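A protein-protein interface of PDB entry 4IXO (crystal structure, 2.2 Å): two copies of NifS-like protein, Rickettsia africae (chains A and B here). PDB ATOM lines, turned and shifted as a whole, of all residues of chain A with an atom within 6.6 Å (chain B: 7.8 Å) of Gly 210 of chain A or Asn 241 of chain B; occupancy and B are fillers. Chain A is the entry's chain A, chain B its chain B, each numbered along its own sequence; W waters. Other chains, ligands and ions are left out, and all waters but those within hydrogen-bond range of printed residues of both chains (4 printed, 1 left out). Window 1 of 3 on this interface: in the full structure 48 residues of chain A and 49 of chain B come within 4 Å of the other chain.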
ATOM      1  N   THR A  77      25.062   2.515  16.787  1.00  0.00           N
ATOM      2  CA  THR A  77      24.556   3.095  15.556  1.00  0.00           C
ATOM      3  C   THR A  77      25.347   4.366  15.291  1.00  0.00           C
ATOM      4  O   THR A  77      26.046   4.882  16.189  1.00  0.00           O
ATOM      5  CB  THR A  77      23.060   3.458  15.685  1.00  0.00           C
ATOM      6  OG1 THR A  77      22.870   4.243  16.867  1.00  0.00           O
ATOM      7  CG2 THR A  77      22.201   2.229  15.813  1.00  0.00           C
ATOM      8  N   SER A  78      25.202   4.905  14.083  1.00  0.00           N
ATOM      9  CA  SER A  78      25.949   6.108  13.710  1.00  0.00           C
ATOM     10  C   SER A  78      25.377   7.331  14.359  1.00  0.00           C
ATOM     11  O   SER A  78      26.068   8.318  14.473  1.00  0.00           O
ATOM     12  CB  SER A  78      25.954   6.292  12.194  1.00  0.00           C
ATOM     13  OG  SER A  78      24.675   6.686  11.706  1.00  0.00           O
ATOM     14  N   SER A  79      24.110   7.276  14.770  1.00  0.00           N
ATOM     15  CA  SER A  79      23.380   8.442  15.245  1.00  0.00           C
ATOM     16  C   SER A  79      22.158   8.040  16.055  1.00  0.00           C
ATOM     17  O   SER A  79      21.693   6.902  15.973  1.00  0.00           O
ATOM     18  CB  SER A  79      22.889   9.256  14.067  1.00  0.00           C
ATOM     19  OG  SER A  79      21.816   8.594  13.397  1.00  0.00           O
ATOM     20  N   GLY A 202      25.888  10.294  21.134  1.00  0.00           N
ATOM     21  CA  GLY A 202      27.147  10.733  21.674  1.00  0.00           C
ATOM     22  C   GLY A 202      27.407  12.230  21.516  1.00  0.00           C
ATOM     23  O   GLY A 202      27.884  12.851  22.446  1.00  0.00           O
ATOM     24  N   HIS A 203      27.077  12.819  20.372  1.00  0.00           N
ATOM     25  CA  HIS A 203      27.457  14.220  20.145  1.00  0.00           C
ATOM     26  C   HIS A 203      26.733  15.209  21.046  1.00  0.00           C
ATOM     27  O   HIS A 203      27.330  16.203  21.470  1.00  0.00           O
ATOM     28  CB  HIS A 203      27.372  14.646  18.681  1.00  0.00           C
ATOM     29  CG  HIS A 203      25.992  14.938  18.189  1.00  0.00           C
ATOM     30  ND1 HIS A 203      25.582  16.212  17.845  1.00  0.00           N
ATOM     31  CD2 HIS A 203      24.964  14.114  17.884  1.00  0.00           C
ATOM     32  CE1 HIS A 203      24.338  16.161  17.411  1.00  0.00           C
ATOM     33  NE2 HIS A 203      23.943  14.900  17.419  1.00  0.00           N
ATOM     34  N   GLY A 207      30.710  13.728  23.242  1.00  0.00           N
ATOM     35  CA  GLY A 207      31.496  12.583  22.780  1.00  0.00           C
ATOM     36  C   GLY A 207      31.865  12.686  21.304  1.00  0.00           C
ATOM     37  O   GLY A 207      32.512  11.799  20.764  1.00  0.00           O
ATOM     38  N   GLY A 208      31.472  13.772  20.664  1.00  0.00           N
ATOM     39  CA  GLY A 208      31.705  13.910  19.229  1.00  0.00           C
ATOM     40  C   GLY A 208      30.650  13.178  18.451  1.00  0.00           C
ATOM     41  O   GLY A 208      29.867  12.396  19.004  1.00  0.00           O
ATOM     42  N   GLN A 209      30.635  13.426  17.146  1.00  0.00           N
ATOM     43  CA  GLN A 209      29.688  12.808  16.264  1.00  0.00           C
ATOM     44  C   GLN A 209      30.094  11.414  15.874  1.00  0.00           C
ATOM     45  O   GLN A 209      31.253  11.102  15.839  1.00  0.00           O
ATOM     46  CB  GLN A 209      29.488  13.685  15.028  1.00  0.00           C
ATOM     47  CG  GLN A 209      28.601  14.869  15.403  1.00  0.00           C
ATOM     48  CD  GLN A 209      28.752  16.105  14.586  1.00  0.00           C
ATOM     49  OE1 GLN A 209      29.607  16.215  13.704  1.00  0.00           O
ATOM     50  NE2 GLN A 209      27.906  17.065  14.886  1.00  0.00           N
ATOM     51  N   GLY A 210      29.103  10.597  15.554  1.00  0.00           N
ATOM     52  CA  GLY A 210      29.337   9.306  14.925  1.00  0.00           C
ATOM     53  C   GLY A 210      29.102   8.115  15.813  1.00  0.00           C
ATOM     54  O   GLY A 210      29.131   6.980  15.333  1.00  0.00           O
ATOM     55  N   GLY A 211      28.888   8.376  17.093  1.00  0.00           N
ATOM     56  CA  GLY A 211      28.631   7.359  18.094  1.00  0.00           C
ATOM     57  C   GLY A 211      27.258   7.555  18.706  1.00  0.00           C
ATOM     58  O   GLY A 211      26.832   8.683  19.024  1.00  0.00           O
ATOM     59  N   ALA A 212      26.546   6.448  18.847  1.00  0.00           N
ATOM     60  CA  ALA A 212      25.202   6.435  19.394  1.00  0.00           C
ATOM     61  C   ALA A 212      24.830   4.976  19.656  1.00  0.00           C
ATOM     62  O   ALA A 212      25.596   4.064  19.352  1.00  0.00           O
ATOM     63  CB  ALA A 212      24.211   7.079  18.428  1.00  0.00           C
ATOM     64  N   ASN A 241      32.546   2.643  13.860  1.00  0.00           N
ATOM     65  CA  ASN A 241      33.260   3.914  14.032  1.00  0.00           C
ATOM     66  C   ASN A 241      33.925   3.930  15.443  1.00  0.00           C
ATOM     67  O   ASN A 241      33.372   4.435  16.421  1.00  0.00           O
ATOM     68  CB  ASN A 241      32.329   5.095  13.825  1.00  0.00           C
ATOM     69  CG  ASN A 241      33.072   6.434  13.798  1.00  0.00           C
ATOM     70  OD1 ASN A 241      34.196   6.545  14.300  1.00  0.00           O
ATOM     71  ND2 ASN A 241      32.426   7.466  13.251  1.00  0.00           N
ATOM     72  N   ALA A 244      34.676   7.286  17.383  1.00  0.00           N
ATOM     73  CA  ALA A 244      33.457   7.910  17.867  1.00  0.00           C
ATOM     74  C   ALA A 244      32.853   7.120  19.028  1.00  0.00           C
ATOM     75  O   ALA A 244      32.336   7.708  19.997  1.00  0.00           O
ATOM     76  CB  ALA A 244      32.429   8.054  16.744  1.00  0.00           C
ATOM     77  N   ILE A 245      32.886   5.798  18.907  1.00  0.00           N
ATOM     78  CA  ILE A 245      32.403   4.918  19.993  1.00  0.00           C
ATOM     79  C   ILE A 245      33.226   5.147  21.276  1.00  0.00           C
ATOM     80  O   ILE A 245      32.662   5.335  22.366  1.00  0.00           O
ATOM     81  CB  ILE A 245      32.412   3.445  19.558  1.00  0.00           C
ATOM     82  CG1 ILE A 245      31.292   3.226  18.526  1.00  0.00           C
ATOM     83  CG2 ILE A 245      32.180   2.509  20.735  1.00  0.00           C
ATOM     84  CD1 ILE A 245      31.414   1.937  17.749  1.00  0.00           C
ATOM     85  N   LEU B  36      29.153  21.620  15.678  1.00  0.00           N
ATOM     86  CA  LEU B  36      28.980  21.435  14.250  1.00  0.00           C
ATOM     87  C   LEU B  36      27.641  20.762  13.912  1.00  0.00           C
ATOM     88  O   LEU B  36      27.563  19.549  13.835  1.00  0.00           O
ATOM     89  CB  LEU B  36      30.145  20.602  13.681  1.00  0.00           C
ATOM     90  CG  LEU B  36      31.558  21.177  13.883  1.00  0.00           C
ATOM     91  CD1 LEU B  36      32.645  20.134  13.657  1.00  0.00           C
ATOM     92  CD2 LEU B  36      31.784  22.366  12.990  1.00  0.00           C
ATOM     93  N   PRO B  38      25.037  21.254  10.810  1.00  0.00           N
ATOM     94  CA  PRO B  38      24.688  21.901   9.565  1.00  0.00           C
ATOM     95  C   PRO B  38      23.223  22.363   9.459  1.00  0.00           C
ATOM     96  O   PRO B  38      22.950  23.280   8.709  1.00  0.00           O
ATOM     97  CB  PRO B  38      24.969  20.840   8.537  1.00  0.00           C
ATOM     98  CG  PRO B  38      26.042  20.018   9.137  1.00  0.00           C
ATOM     99  CD  PRO B  38      25.681  19.953  10.586  1.00  0.00           C
ATOM    100  N   ILE B  52      30.580  20.681   4.915  1.00  0.00           N
ATOM    101  CA  ILE B  52      30.086  19.499   4.219  1.00  0.00           C
ATOM    102  C   ILE B  52      29.823  19.762   2.731  1.00  0.00           C
ATOM    103  O   ILE B  52      30.061  18.862   1.924  1.00  0.00           O
ATOM    104  CB  ILE B  52      28.887  18.808   4.897  1.00  0.00           C
ATOM    105  CG1 ILE B  52      27.607  19.616   4.802  1.00  0.00           C
ATOM    106  CG2 ILE B  52      29.233  18.491   6.358  1.00  0.00           C
ATOM    107  CD1 ILE B  52      26.411  18.881   5.380  1.00  0.00           C
ATOM    108  N   PHE B  76      25.702  11.715   1.848  1.00  0.00           N
ATOM    109  CA  PHE B  76      26.632  11.253   2.870  1.00  0.00           C
ATOM    110  C   PHE B  76      25.978  10.211   3.788  1.00  0.00           C
ATOM    111  O   PHE B  76      24.915  10.456   4.364  1.00  0.00           O
ATOM    112  CB  PHE B  76      27.170  12.416   3.704  1.00  0.00           C
ATOM    113  CG  PHE B  76      28.033  13.375   2.916  1.00  0.00           C
ATOM    114  CD1 PHE B  76      29.186  12.932   2.290  1.00  0.00           C
ATOM    115  CD2 PHE B  76      27.729  14.706   2.868  1.00  0.00           C
ATOM    116  CE1 PHE B  76      29.968  13.806   1.546  1.00  0.00           C
ATOM    117  CE2 PHE B  76      28.504  15.588   2.148  1.00  0.00           C
ATOM    118  CZ  PHE B  76      29.619  15.137   1.478  1.00  0.00           C
ATOM    119  N   THR B  77      26.627   9.061   3.894  1.00  0.00           N
ATOM    120  CA  THR B  77      26.224   7.967   4.746  1.00  0.00           C
ATOM    121  C   THR B  77      27.333   7.727   5.780  1.00  0.00           C
ATOM    122  O   THR B  77      28.437   8.259   5.653  1.00  0.00           O
ATOM    123  CB  THR B  77      26.033   6.681   3.935  1.00  0.00           C
ATOM    124  OG1 THR B  77      27.203   6.453   3.170  1.00  0.00           O
ATOM    125  CG2 THR B  77      24.887   6.794   2.989  1.00  0.00           C
ATOM    126  N   SER B  78      27.028   6.929   6.803  1.00  0.00           N
ATOM    127  CA  SER B  78      27.971   6.689   7.867  1.00  0.00           C
ATOM    128  C   SER B  78      29.056   5.750   7.401  1.00  0.00           C
ATOM    129  O   SER B  78      30.107   5.727   7.983  1.00  0.00           O
ATOM    130  CB  SER B  78      27.284   6.107   9.092  1.00  0.00           C
ATOM    131  OG  SER B  78      26.861   4.761   8.878  1.00  0.00           O
ATOM    132  N   GLN B 209      37.044   7.035  10.055  1.00  0.00           N
ATOM    133  CA  GLN B 209      35.756   6.361  10.005  1.00  0.00           C
ATOM    134  C   GLN B 209      34.641   7.352  10.130  1.00  0.00           C
ATOM    135  O   GLN B 209      34.799   8.394  10.746  1.00  0.00           O
ATOM    136  CB  GLN B 209      35.684   5.306  11.124  1.00  0.00           C
ATOM    137  CG  GLN B 209      36.478   4.099  10.707  1.00  0.00           C
ATOM    138  CD  GLN B 209      37.059   3.267  11.810  1.00  0.00           C
ATOM    139  OE1 GLN B 209      36.921   3.545  13.005  1.00  0.00           O
ATOM    140  NE2 GLN B 209      37.719   2.199  11.398  1.00  0.00           N
ATOM    141  N   GLY B 210      33.511   6.996   9.553  1.00  0.00           N
ATOM    142  CA  GLY B 210      32.253   7.704   9.781  1.00  0.00           C
ATOM    143  C   GLY B 210      31.757   8.515   8.620  1.00  0.00           C
ATOM    144  O   GLY B 210      30.651   9.068   8.670  1.00  0.00           O
ATOM    145  N   GLY B 211      32.593   8.605   7.587  1.00  0.00           N
ATOM    146  CA  GLY B 211      32.287   9.329   6.359  1.00  0.00           C
ATOM    147  C   GLY B 211      32.276   8.378   5.172  1.00  0.00           C
ATOM    148  O   GLY B 211      33.136   7.525   5.034  1.00  0.00           O
ATOM    149  N   ALA B 212      31.263   8.536   4.327  1.00  0.00           N
ATOM    150  CA  ALA B 212      31.077   7.702   3.142  1.00  0.00           C
ATOM    151  C   ALA B 212      29.996   8.348   2.308  1.00  0.00           C
ATOM    152  O   ALA B 212      29.427   9.355   2.698  1.00  0.00           O
ATOM    153  CB  ALA B 212      30.669   6.291   3.531  1.00  0.00           C
ATOM    154  N   ARG B 236      18.635  10.906   3.731  1.00  0.00           N
ATOM    155  CA  ARG B 236      19.403  10.263   4.806  1.00  0.00           C
ATOM    156  C   ARG B 236      19.464  11.200   6.012  1.00  0.00           C
ATOM    157  O   ARG B 236      20.306  12.100   6.083  1.00  0.00           O
ATOM    158  CB  ARG B 236      20.807   9.912   4.284  1.00  0.00           C
ATOM    159  CG  ARG B 236      21.563   8.847   5.039  1.00  0.00           C
ATOM    160  CD  ARG B 236      22.230   9.435   6.243  1.00  0.00           C
ATOM    161  NE  ARG B 236      22.875   8.437   7.075  1.00  0.00           N
ATOM    162  CZ  ARG B 236      23.435   8.722   8.248  1.00  0.00           C
ATOM    163  NH1 ARG B 236      23.465   9.976   8.703  1.00  0.00           N
ATOM    164  NH2 ARG B 236      23.958   7.762   8.977  1.00  0.00           N
ATOM    165  N   GLY B 238      19.501  12.362  10.176  1.00  0.00           N
ATOM    166  CA  GLY B 238      20.449  12.208  11.256  1.00  0.00           C
ATOM    167  C   GLY B 238      21.435  13.345  11.149  1.00  0.00           C
ATOM    168  O   GLY B 238      21.741  13.825  10.048  1.00  0.00           O
ATOM    169  N   THR B 239      21.934  13.792  12.298  1.00  0.00           N
ATOM    170  CA  THR B 239      22.888  14.870  12.311  1.00  0.00           C
ATOM    171  C   THR B 239      24.134  14.381  11.568  1.00  0.00           C
ATOM    172  O   THR B 239      24.658  13.305  11.847  1.00  0.00           O
ATOM    173  CB  THR B 239      23.221  15.309  13.741  1.00  0.00           C
ATOM    174  OG1 THR B 239      22.010  15.718  14.402  1.00  0.00           O
ATOM    175  CG2 THR B 239      24.202  16.461  13.732  1.00  0.00           C
ATOM    176  N   GLU B 240      24.588  15.183  10.611  1.00  0.00           N
ATOM    177  CA  GLU B 240      25.723  14.810   9.776  1.00  0.00           C
ATOM    178  C   GLU B 240      26.978  14.726  10.648  1.00  0.00           C
ATOM    179  O   GLU B 240      27.163  15.553  11.563  1.00  0.00           O
ATOM    180  CB  GLU B 240      25.930  15.825   8.639  1.00  0.00           C
ATOM    181  CG  GLU B 240      24.701  16.083   7.759  1.00  0.00           C
ATOM    182  CD  GLU B 240      23.813  17.244   8.226  1.00  0.00           C
ATOM    183  OE1 GLU B 240      23.819  17.574   9.463  1.00  0.00           O
ATOM    184  OE2 GLU B 240      23.116  17.826   7.349  1.00  0.00           O
ATOM    185  N   ASN B 241      27.810  13.715  10.375  1.00  0.00           N
ATOM    186  CA  ASN B 241      29.084  13.553  11.051  1.00  0.00           C
ATOM    187  C   ASN B 241      30.105  14.452  10.345  1.00  0.00           C
ATOM    188  O   ASN B 241      30.862  14.037   9.434  1.00  0.00           O
ATOM    189  CB  ASN B 241      29.524  12.080  11.045  1.00  0.00           C
ATOM    190  CG  ASN B 241      30.775  11.847  11.871  1.00  0.00           C
ATOM    191  OD1 ASN B 241      31.527  12.786  12.157  1.00  0.00           O
ATOM    192  ND2 ASN B 241      31.025  10.578  12.248  1.00  0.00           N
ATOM    193  N   VAL B 242      30.109  15.706  10.770  1.00  0.00           N
ATOM    194  CA  VAL B 242      30.835  16.741  10.058  1.00  0.00           C
ATOM    195  C   VAL B 242      32.347  16.499  10.013  1.00  0.00           C
ATOM    196  O   VAL B 242      32.975  16.692   8.957  1.00  0.00           O
ATOM    197  CB  VAL B 242      30.502  18.136  10.649  1.00  0.00           C
ATOM    198  CG1 VAL B 242      31.342  19.224   9.985  1.00  0.00           C
ATOM    199  CG2 VAL B 242      29.034  18.436  10.437  1.00  0.00           C
ATOM    200  N   LEU B 243      32.928  16.107  11.137  1.00  0.00           N
ATOM    201  CA  LEU B 243      34.370  15.860  11.229  1.00  0.00           C
ATOM    202  C   LEU B 243      34.802  14.721  10.294  1.00  0.00           C
ATOM    203  O   LEU B 243      35.809  14.817   9.619  1.00  0.00           O
ATOM    204  CB  LEU B 243      34.792  15.512  12.662  1.00  0.00           C
ATOM    205  CG  LEU B 243      34.741  16.619  13.734  1.00  0.00           C
ATOM    206  CD1 LEU B 243      35.346  16.093  15.013  1.00  0.00           C
ATOM    207  CD2 LEU B 243      35.485  17.884  13.359  1.00  0.00           C
ATOM    208  N   ALA B 244      34.023  13.656  10.271  1.00  0.00           N
ATOM    209  CA  ALA B 244      34.315  12.528   9.384  1.00  0.00           C
ATOM    210  C   ALA B 244      34.140  12.891   7.926  1.00  0.00           C
ATOM    211  O   ALA B 244      34.911  12.475   7.066  1.00  0.00           O
ATOM    212  CB  ALA B 244      33.423  11.336   9.741  1.00  0.00           C
ATOM    213  N   ILE B 245      33.117  13.675   7.634  1.00  0.00           N
ATOM    214  CA  ILE B 245      32.883  14.135   6.260  1.00  0.00           C
ATOM    215  C   ILE B 245      34.052  15.023   5.799  1.00  0.00           C
ATOM    216  O   ILE B 245      34.599  14.848   4.706  1.00  0.00           O
ATOM    217  CB  ILE B 245      31.527  14.873   6.146  1.00  0.00           C
ATOM    218  CG1 ILE B 245      30.397  13.844   6.253  1.00  0.00           C
ATOM    219  CG2 ILE B 245      31.398  15.607   4.816  1.00  0.00           C
ATOM    220  CD1 ILE B 245      29.018  14.437   6.511  1.00  0.00           C
ATOM    221  N   ALA B 246      34.430  15.962   6.660  1.00  0.00           N
ATOM    222  CA  ALA B 246      35.565  16.833   6.414  1.00  0.00           C
ATOM    223  C   ALA B 246      36.826  16.004   6.151  1.00  0.00           C
ATOM    224  O   ALA B 246      37.509  16.232   5.165  1.00  0.00           O
ATOM    225  CB  ALA B 246      35.769  17.758   7.588  1.00  0.00           C
ATOM    226  N   GLY B 247      37.107  15.014   7.000  1.00  0.00           N
ATOM    227  CA  GLY B 247      38.253  14.121   6.768  1.00  0.00           C
ATOM    228  C   GLY B 247      38.188  13.367   5.438  1.00  0.00           C
ATOM    229  O   GLY B 247      39.174  13.263   4.726  1.00  0.00           O
ATOM    230  N   PHE B 248      37.000  12.848   5.126  1.00  0.00           N
ATOM    231  CA  PHE B 248      36.717  12.158   3.876  1.00  0.00           C
ATOM    232  C   PHE B 248      37.030  13.044   2.673  1.00  0.00           C
ATOM    233  O   PHE B 248      37.678  12.617   1.699  1.00  0.00           O
ATOM    234  CB  PHE B 248      35.241  11.752   3.910  1.00  0.00           C
ATOM    235  CG  PHE B 248      34.767  10.928   2.764  1.00  0.00           C
ATOM    236  CD1 PHE B 248      35.614  10.130   2.034  1.00  0.00           C
ATOM    237  CD2 PHE B 248      33.411  10.921   2.442  1.00  0.00           C
ATOM    238  CE1 PHE B 248      35.132   9.336   1.004  1.00  0.00           C
ATOM    239  CE2 PHE B 248      32.925  10.132   1.424  1.00  0.00           C
ATOM    240  CZ  PHE B 248      33.791   9.336   0.704  1.00  0.00           C
HETATM  241  O   HOH W   1      36.931   5.695  14.220  1.00  0.00           O
HETATM  242  O   HOH W   2      31.825  15.215  13.715  1.00  0.00           O
HETATM  243  O   HOH W   3      21.423   8.405  10.655  1.00  0.00           O
HETATM  244  O   HOH W   4      33.544  10.145  13.497  1.00  0.00           O
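Ser 78 of chain A touches its own counterpart, Ser 78 of chain B. Gln 209 of chain A touches Asn 241 of chain B, and with the chains exchanged Asn 241 of chain A touches Gln 209 of chain B. Gly 210 of chain A touches Asn 241 of chain B, and with the chains exchanged Asn 241 of chain A touches Gly 210 of chain B. Asn 241 of chain A touches its own counterpart, Asn 241 of chain B. Of the 12 pairs that touch across the chains among the printed residues, 6 have their exchanged pair printed and touching as well.
Hydrophobic or aromatic side chains of chain A within 4 Å of the printed part of chain B: His 203. Hydrophobic or aromatic side chains of chain B that line the printed part of chain A: Val 242.
N of Ala 244 of chain B is in hydrogen-bond range of OD1 of Asn 241 of chain B (3.2 Å). OD1 of Asn 241 of chain A is in hydrogen-bond range of N of Ala 244 of chain A (3.2 Å). O of Gly 208 of chain A sits at hydrogen-bond distance from N of His 203 of chain A, 3.1 Å away.
Of chain B, only Asn 241 comes within 4 Å of Gly 210 of chain A. Asn 241 of chain B touches just these residues of chain A: Gln 209, Gly 210 and Asn 241. Of the printed residues of chain A, Arg 236 of chain B touches Ser 78 (3.0 Å). Of the printed residues of chain B, Ser 78 of chain A touches Ser 78 (3.4 Å) and Arg 236 (3.0 Å). Gly 207 of chain A touches none of the printed residues of chain B. Pro 38 of chain B touches none of the printed residues of chain A. The nearest residue of chain B that does not touch Gly 210 of chain A is Gly 210 of chain B (6.1 Å). The nearest residue of chain A that does not touch Asn 241 of chain B is Ala 244 of chain A (5.3 Å). The nearest printed residue of chain A that does not touch Gly 210 of chain B is Gly 210 of chain A (6.1 Å).
Among the printed residues, pairs that only touch across the chains: Ser 78 of chain A with Ser 78 of chain B, His 203 of chain A with Thr 239 of chain B, Gln 209 of chain A with Thr 239 of chain B, Gln 209 of chain A with Asn 241 of chain B, Gly 210 of chain A with Asn 241 of chain B, Asn 241 of chain A with Gln 209 of chain B, Asn 241 of chain A with Gly 210 of chain B and Asn 241 of chain A with Asn 241 of chain B.
Water W2 lies within hydrogen-bond range of the side-chain amide oxygen (OE1) of Gln 209 of chain A, the side-chain amide oxygen (OD1) of Asn 241 of chain B, the backbone NH (N) of Leu 243 of chain B and the backbone NH (N) of Val 242 of chain B. Water W1 bridges the side-chain amide oxygen (OE1) of Gln 209 of chain B (2.5 Å) and the side-chain amide oxygen (OD1) of Asn 241 of chain A (2.9 Å). Water W3 bridges OG of Ser 79 of chain A (2.8 Å) and NH2 of Arg 236 of chain B (3.1 Å). Water W4 lies within hydrogen-bond range of ND2 of Asn 241 of chain B (2.8 Å), ND2 of Asn 241 of chain A (2.9 Å), O of Gln 209 of chain A (3.4 Å) and O of Gln 209 of chain B (3.5 Å).
The guanidinium group (NH2) of Arg 236 of chain B is in hydrogen-bond range of the side-chain hydroxyl (OG) of Ser 78 of chain A, 3.0 Å away. The backbone carbonyl oxygen of Leu 36 of chain B is in hydrogen-bond range of the side-chain amide nitrogen of Gln 209 of chain A, at 2.7 Å. OE1 of Gln 209 of chain A lies close to O of Glu 240 of chain B, 3.3 Å away. OE1 of Gln 209 of chain A is in hydrogen-bond range of N of Val 242 of chain B.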
